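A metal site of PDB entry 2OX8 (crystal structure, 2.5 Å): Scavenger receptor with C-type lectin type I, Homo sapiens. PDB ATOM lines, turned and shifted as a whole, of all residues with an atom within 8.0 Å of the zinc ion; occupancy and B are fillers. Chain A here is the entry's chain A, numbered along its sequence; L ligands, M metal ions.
OE2 of Glu 129 lies close to OH of Tyr 17 (3.2 Å).
N of Glu 129 is in hydrogen-bond range of O of His 39, 2.9 Å away.
The side-chain carboxylate of Glu 48 sits close to the side-chain hydroxyl of Tyr 17 (2.6 Å).
The backbone NH (N) of Asn 44 is in hydrogen-bond range of the side-chain carboxylate (OE2) of Glu 48 (3.1 Å).
The backbone NH of Glu 48 lies within hydrogen-bond range of the side-chain hydroxyl of Thr 45.
The zinc ion is bound by the side-chain carboxylate (OE2) of Glu 129, the side-chain carboxylate (OE1) of Glu 48, a chlorine (CL1) of the ligand and the backbone carbonyl oxygen (O) of Phe 42.
The zinc ion has four donor atoms within binding distance.
Residues that only touch the zinc ion: Tyr 17 (3.6 Å).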
ATOM      1  N   PHE A  12      -4.241 -19.719 -11.477  1.00  0.00           N
ATOM      2  CA  PHE A  12      -5.207 -19.729 -12.562  1.00  0.00           C
ATOM      3  C   PHE A  12      -6.517 -20.097 -11.901  1.00  0.00           C
ATOM      4  O   PHE A  12      -6.640 -21.153 -11.282  1.00  0.00           O
ATOM      5  CB  PHE A  12      -4.859 -20.805 -13.600  1.00  0.00           C
ATOM      6  CG  PHE A  12      -5.914 -20.961 -14.677  1.00  0.00           C
ATOM      7  CD1 PHE A  12      -6.006 -20.051 -15.721  1.00  0.00           C
ATOM      8  CD2 PHE A  12      -6.825 -22.015 -14.615  1.00  0.00           C
ATOM      9  CE1 PHE A  12      -6.992 -20.171 -16.705  1.00  0.00           C
ATOM     10  CE2 PHE A  12      -7.816 -22.142 -15.589  1.00  0.00           C
ATOM     11  CZ  PHE A  12      -7.896 -21.216 -16.634  1.00  0.00           C
ATOM     12  N   ASP A  14      -8.877 -20.550  -9.184  1.00  0.00           N
ATOM     13  CA  ASP A  14      -8.715 -20.591  -7.726  1.00  0.00           C
ATOM     14  C   ASP A  14      -7.679 -21.635  -7.326  1.00  0.00           C
ATOM     15  O   ASP A  14      -7.640 -22.082  -6.181  1.00  0.00           O
ATOM     16  CB  ASP A  14     -10.051 -20.912  -7.056  1.00  0.00           C
ATOM     17  CG  ASP A  14     -10.537 -22.318  -7.337  1.00  0.00           C
ATOM     18  OD1 ASP A  14     -10.180 -22.894  -8.393  1.00  0.00           O
ATOM     19  OD2 ASP A  14     -11.304 -22.857  -6.509  1.00  0.00           O
ATOM     20  N   LYS A  15      -6.830 -21.993  -8.278  1.00  0.00           N
ATOM     21  CA  LYS A  15      -5.840 -23.024  -8.036  1.00  0.00           C
ATOM     22  C   LYS A  15      -4.386 -22.604  -8.240  1.00  0.00           C
ATOM     23  O   LYS A  15      -4.051 -21.802  -9.140  1.00  0.00           O
ATOM     24  CB  LYS A  15      -6.124 -24.215  -8.943  1.00  0.00           C
ATOM     25  CG  LYS A  15      -7.563 -24.660  -8.920  1.00  0.00           C
ATOM     26  CD  LYS A  15      -7.837 -25.668 -10.012  1.00  0.00           C
ATOM     27  CE  LYS A  15      -9.169 -26.323  -9.802  1.00  0.00           C
ATOM     28  NZ  LYS A  15     -10.200 -25.285  -9.850  1.00  0.00           N
ATOM     29  N   TYR A  17      -0.643 -23.876  -9.099  1.00  0.00           N
ATOM     30  CA  TYR A  17       0.051 -24.926  -9.837  1.00  0.00           C
ATOM     31  C   TYR A  17       1.563 -24.885  -9.606  1.00  0.00           C
ATOM     32  O   TYR A  17       2.160 -23.836  -9.440  1.00  0.00           O
ATOM     33  CB  TYR A  17      -0.241 -24.789 -11.331  1.00  0.00           C
ATOM     34  CG  TYR A  17      -1.689 -24.938 -11.711  1.00  0.00           C
ATOM     35  CD1 TYR A  17      -2.605 -23.944 -11.433  1.00  0.00           C
ATOM     36  CD2 TYR A  17      -2.149 -26.104 -12.323  1.00  0.00           C
ATOM     37  CE1 TYR A  17      -3.955 -24.099 -11.761  1.00  0.00           C
ATOM     38  CE2 TYR A  17      -3.488 -26.278 -12.640  1.00  0.00           C
ATOM     39  CZ  TYR A  17      -4.386 -25.261 -12.366  1.00  0.00           C
ATOM     40  OH  TYR A  17      -5.717 -25.408 -12.715  1.00  0.00           O
ATOM     41  N   HIS A  39      -1.797 -32.561  -5.472  1.00  0.00           N
ATOM     42  CA  HIS A  39      -1.778 -33.809  -6.189  1.00  0.00           C
ATOM     43  C   HIS A  39      -1.441 -33.505  -7.627  1.00  0.00           C
ATOM     44  O   HIS A  39      -1.619 -32.369  -8.066  1.00  0.00           O
ATOM     45  CB  HIS A  39      -3.173 -34.440  -6.156  1.00  0.00           C
ATOM     46  CG  HIS A  39      -4.265 -33.486  -6.515  1.00  0.00           C
ATOM     47  ND1 HIS A  39      -4.462 -33.025  -7.799  1.00  0.00           N
ATOM     48  CD2 HIS A  39      -5.178 -32.847  -5.739  1.00  0.00           C
ATOM     49  CE1 HIS A  39      -5.449 -32.144  -7.808  1.00  0.00           C
ATOM     50  NE2 HIS A  39      -5.900 -32.018  -6.572  1.00  0.00           N
ATOM     51  N   LEU A  40      -0.937 -34.506  -8.343  1.00  0.00           N
ATOM     52  CA  LEU A  40      -0.624 -34.315  -9.731  1.00  0.00           C
ATOM     53  C   LEU A  40      -1.901 -33.685 -10.333  1.00  0.00           C
ATOM     54  O   LEU A  40      -3.040 -34.081 -10.027  1.00  0.00           O
ATOM     55  CB  LEU A  40      -0.243 -35.655 -10.362  1.00  0.00           C
ATOM     56  CG  LEU A  40       1.204 -36.123 -10.028  1.00  0.00           C
ATOM     57  CD1 LEU A  40       1.366 -37.611 -10.287  1.00  0.00           C
ATOM     58  CD2 LEU A  40       2.217 -35.317 -10.856  1.00  0.00           C
ATOM     59  N   VAL A  41      -1.672 -32.664 -11.159  1.00  0.00           N
ATOM     60  CA  VAL A  41      -2.712 -31.877 -11.792  1.00  0.00           C
ATOM     61  C   VAL A  41      -3.850 -32.656 -12.495  1.00  0.00           C
ATOM     62  O   VAL A  41      -3.627 -33.713 -13.082  1.00  0.00           O
ATOM     63  CB  VAL A  41      -2.058 -30.906 -12.802  1.00  0.00           C
ATOM     64  CG1 VAL A  41      -1.488 -31.677 -13.972  1.00  0.00           C
ATOM     65  CG2 VAL A  41      -3.034 -29.880 -13.276  1.00  0.00           C
ATOM     66  N   PHE A  42      -5.064 -32.117 -12.391  1.00  0.00           N
ATOM     67  CA  PHE A  42      -6.251 -32.685 -13.044  1.00  0.00           C
ATOM     68  C   PHE A  42      -6.591 -31.605 -14.069  1.00  0.00           C
ATOM     69  O   PHE A  42      -6.576 -30.413 -13.743  1.00  0.00           O
ATOM     70  CB  PHE A  42      -7.450 -32.808 -12.099  1.00  0.00           C
ATOM     71  CG  PHE A  42      -7.266 -33.766 -10.980  1.00  0.00           C
ATOM     72  CD1 PHE A  42      -7.997 -33.623  -9.821  1.00  0.00           C
ATOM     73  CD2 PHE A  42      -6.334 -34.796 -11.065  1.00  0.00           C
ATOM     74  CE1 PHE A  42      -7.806 -34.490  -8.739  1.00  0.00           C
ATOM     75  CE2 PHE A  42      -6.136 -35.669  -9.993  1.00  0.00           C
ATOM     76  CZ  PHE A  42      -6.876 -35.505  -8.815  1.00  0.00           C
ATOM     77  N   ILE A  43      -6.873 -32.002 -15.304  1.00  0.00           N
ATOM     78  CA  ILE A  43      -7.222 -31.030 -16.331  1.00  0.00           C
ATOM     79  C   ILE A  43      -8.669 -31.274 -16.744  1.00  0.00           C
ATOM     80  O   ILE A  43      -8.964 -32.226 -17.466  1.00  0.00           O
ATOM     81  CB  ILE A  43      -6.274 -31.155 -17.529  1.00  0.00           C
ATOM     82  CG1 ILE A  43      -4.864 -30.814 -17.079  1.00  0.00           C
ATOM     83  CG2 ILE A  43      -6.731 -30.254 -18.661  1.00  0.00           C
ATOM     84  CD1 ILE A  43      -3.789 -31.339 -17.967  1.00  0.00           C
ATOM     85  N   ASN A  44      -9.573 -30.417 -16.286  1.00  0.00           N
ATOM     86  CA  ASN A  44     -10.984 -30.620 -16.565  1.00  0.00           C
ATOM     87  C   ASN A  44     -11.736 -29.680 -17.514  1.00  0.00           C
ATOM     88  O   ASN A  44     -12.959 -29.747 -17.597  1.00  0.00           O
ATOM     89  CB  ASN A  44     -11.737 -30.706 -15.247  1.00  0.00           C
ATOM     90  CG  ASN A  44     -11.402 -31.960 -14.502  1.00  0.00           C
ATOM     91  OD1 ASN A  44     -11.595 -33.065 -15.010  1.00  0.00           O
ATOM     92  ND2 ASN A  44     -10.891 -31.822 -13.287  1.00  0.00           N
ATOM     93  N   THR A  45     -11.011 -28.840 -18.239  1.00  0.00           N
ATOM     94  CA  THR A  45     -11.650 -27.935 -19.166  1.00  0.00           C
ATOM     95  C   THR A  45     -10.604 -27.535 -20.168  1.00  0.00           C
ATOM     96  O   THR A  45      -9.421 -27.560 -19.864  1.00  0.00           O
ATOM     97  CB  THR A  45     -12.153 -26.656 -18.460  1.00  0.00           C
ATOM     98  OG1 THR A  45     -11.059 -26.046 -17.751  1.00  0.00           O
ATOM     99  CG2 THR A  45     -13.274 -26.988 -17.486  1.00  0.00           C
ATOM    100  N   GLU A  48      -8.475 -24.529 -19.065  1.00  0.00           N
ATOM    101  CA  GLU A  48      -7.398 -24.858 -18.146  1.00  0.00           C
ATOM    102  C   GLU A  48      -6.254 -25.443 -18.986  1.00  0.00           C
ATOM    103  O   GLU A  48      -5.115 -25.014 -18.871  1.00  0.00           O
ATOM    104  CB  GLU A  48      -7.857 -25.857 -17.070  1.00  0.00           C
ATOM    105  CG  GLU A  48      -6.794 -26.210 -16.028  1.00  0.00           C
ATOM    106  CD  GLU A  48      -7.254 -27.240 -15.000  1.00  0.00           C
ATOM    107  OE1 GLU A  48      -6.515 -27.516 -14.026  1.00  0.00           O
ATOM    108  OE2 GLU A  48      -8.346 -27.787 -15.150  1.00  0.00           O
ATOM    109  N   GLN A  49      -6.583 -26.401 -19.835  1.00  0.00           N
ATOM    110  CA  GLN A  49      -5.593 -27.036 -20.708  1.00  0.00           C
ATOM    111  C   GLN A  49      -4.831 -25.998 -21.542  1.00  0.00           C
ATOM    112  O   GLN A  49      -3.632 -26.115 -21.725  1.00  0.00           O
ATOM    113  CB  GLN A  49      -6.262 -28.069 -21.624  1.00  0.00           C
ATOM    114  CG  GLN A  49      -5.397 -28.627 -22.734  1.00  0.00           C
ATOM    115  CD  GLN A  49      -4.248 -29.465 -22.228  1.00  0.00           C
ATOM    116  OE1 GLN A  49      -4.452 -30.541 -21.661  1.00  0.00           O
ATOM    117  NE2 GLN A  49      -3.017 -28.987 -22.447  1.00  0.00           N
ATOM    118  N   TRP A  51      -4.256 -22.925 -20.693  1.00  0.00           N
ATOM    119  CA  TRP A  51      -3.444 -22.131 -19.773  1.00  0.00           C
ATOM    120  C   TRP A  51      -2.200 -22.892 -19.381  1.00  0.00           C
ATOM    121  O   TRP A  51      -1.097 -22.360 -19.371  1.00  0.00           O
ATOM    122  CB  TRP A  51      -4.225 -21.796 -18.513  1.00  0.00           C
ATOM    123  CG  TRP A  51      -3.405 -21.060 -17.508  1.00  0.00           C
ATOM    124  CD1 TRP A  51      -3.089 -19.729 -17.540  1.00  0.00           C
ATOM    125  CD2 TRP A  51      -2.759 -21.592 -16.338  1.00  0.00           C
ATOM    126  NE1 TRP A  51      -2.298 -19.407 -16.463  1.00  0.00           N
ATOM    127  CE2 TRP A  51      -2.071 -20.524 -15.708  1.00  0.00           C
ATOM    128  CE3 TRP A  51      -2.701 -22.871 -15.758  1.00  0.00           C
ATOM    129  CZ2 TRP A  51      -1.325 -20.701 -14.531  1.00  0.00           C
ATOM    130  CZ3 TRP A  51      -1.950 -23.040 -14.592  1.00  0.00           C
ATOM    131  CH2 TRP A  51      -1.274 -21.954 -13.993  1.00  0.00           C
ATOM    132  N   ILE A  52      -2.400 -24.167 -19.031  1.00  0.00           N
ATOM    133  CA  ILE A  52      -1.301 -25.018 -18.630  1.00  0.00           C
ATOM    134  C   ILE A  52      -0.209 -25.045 -19.687  1.00  0.00           C
ATOM    135  O   ILE A  52       0.974 -25.004 -19.367  1.00  0.00           O
ATOM    136  CB  ILE A  52      -1.818 -26.436 -18.334  1.00  0.00           C
ATOM    137  CG1 ILE A  52      -2.506 -26.440 -16.968  1.00  0.00           C
ATOM    138  CG2 ILE A  52      -0.683 -27.452 -18.368  1.00  0.00           C
ATOM    139  CD1 ILE A  52      -3.162 -27.763 -16.586  1.00  0.00           C
ATOM    140  N   TRP A  77      -8.788 -39.695 -13.032  1.00  0.00           N
ATOM    141  CA  TRP A  77      -7.956 -38.721 -12.357  1.00  0.00           C
ATOM    142  C   TRP A  77      -7.792 -39.293 -10.952  1.00  0.00           C
ATOM    143  O   TRP A  77      -8.685 -40.013 -10.493  1.00  0.00           O
ATOM    144  CB  TRP A  77      -8.675 -37.387 -12.291  1.00  0.00           C
ATOM    145  CG  TRP A  77      -8.862 -36.748 -13.619  1.00  0.00           C
ATOM    146  CD1 TRP A  77     -10.051 -36.509 -14.250  1.00  0.00           C
ATOM    147  CD2 TRP A  77      -7.840 -36.206 -14.459  1.00  0.00           C
ATOM    148  NE1 TRP A  77      -9.819 -35.845 -15.434  1.00  0.00           N
ATOM    149  CE2 TRP A  77      -8.477 -35.649 -15.592  1.00  0.00           C
ATOM    150  CE3 TRP A  77      -6.438 -36.138 -14.371  1.00  0.00           C
ATOM    151  CZ2 TRP A  77      -7.774 -35.038 -16.621  1.00  0.00           C
ATOM    152  CZ3 TRP A  77      -5.743 -35.521 -15.410  1.00  0.00           C
ATOM    153  CH2 TRP A  77      -6.406 -34.980 -16.519  1.00  0.00           C
ATOM    154  N   GLU A 129      -0.990 -29.529  -8.232  1.00  0.00           N
ATOM    155  CA  GLU A 129      -2.125 -28.643  -8.220  1.00  0.00           C
ATOM    156  C   GLU A 129      -2.870 -28.734  -6.882  1.00  0.00           C
ATOM    157  O   GLU A 129      -2.853 -29.792  -6.235  1.00  0.00           O
ATOM    158  CB  GLU A 129      -3.044 -29.044  -9.381  1.00  0.00           C
ATOM    159  CG  GLU A 129      -4.408 -28.350  -9.456  1.00  0.00           C
ATOM    160  CD  GLU A 129      -5.340 -29.001 -10.478  1.00  0.00           C
ATOM    161  OE1 GLU A 129      -5.606 -30.205 -10.359  1.00  0.00           O
ATOM    162  OE2 GLU A 129      -5.818 -28.296 -11.393  1.00  0.00           O
ATOM    163  N   LYS A 130      -3.480 -27.630  -6.477  1.00  0.00           N
ATOM    164  CA  LYS A 130      -4.279 -27.592  -5.255  1.00  0.00           C
ATOM    165  C   LYS A 130      -5.224 -26.395  -5.332  1.00  0.00           C
ATOM    166  O   LYS A 130      -4.829 -25.306  -5.745  1.00  0.00           O
ATOM    167  CB  LYS A 130      -3.412 -27.520  -3.996  1.00  0.00           C
ATOM    168  CG  LYS A 130      -2.476 -26.326  -3.919  1.00  0.00           C
ATOM    169  CD  LYS A 130      -1.712 -26.356  -2.593  1.00  0.00           C
ATOM    170  CE  LYS A 130      -0.467 -25.479  -2.610  1.00  0.00           C
ATOM    171  NZ  LYS A 130       0.356 -25.802  -1.409  1.00  0.00           N
ATOM    172  N   ASP A 131      -6.479 -26.616  -4.958  1.00  0.00           N
ATOM    173  CA  ASP A 131      -7.506 -25.591  -4.985  1.00  0.00           C
ATOM    174  C   ASP A 131      -7.564 -24.887  -3.622  1.00  0.00           C
ATOM    175  O   ASP A 131      -7.742 -25.525  -2.595  1.00  0.00           O
ATOM    176  CB  ASP A 131      -8.854 -26.261  -5.346  1.00  0.00           C
ATOM    177  CG  ASP A 131     -10.045 -25.356  -5.139  1.00  0.00           C
ATOM    178  OD1 ASP A 131     -10.263 -24.865  -4.009  1.00  0.00           O
ATOM    179  OD2 ASP A 131     -10.798 -25.132  -6.097  1.00  0.00           O
HETATM  180 CL1  LIG L   1      -9.132 -29.334 -12.306  1.00  0.00          CL
HETATM  181 ZN    ZN M   1      -7.151 -28.738 -12.607  1.00  0.00          ZN
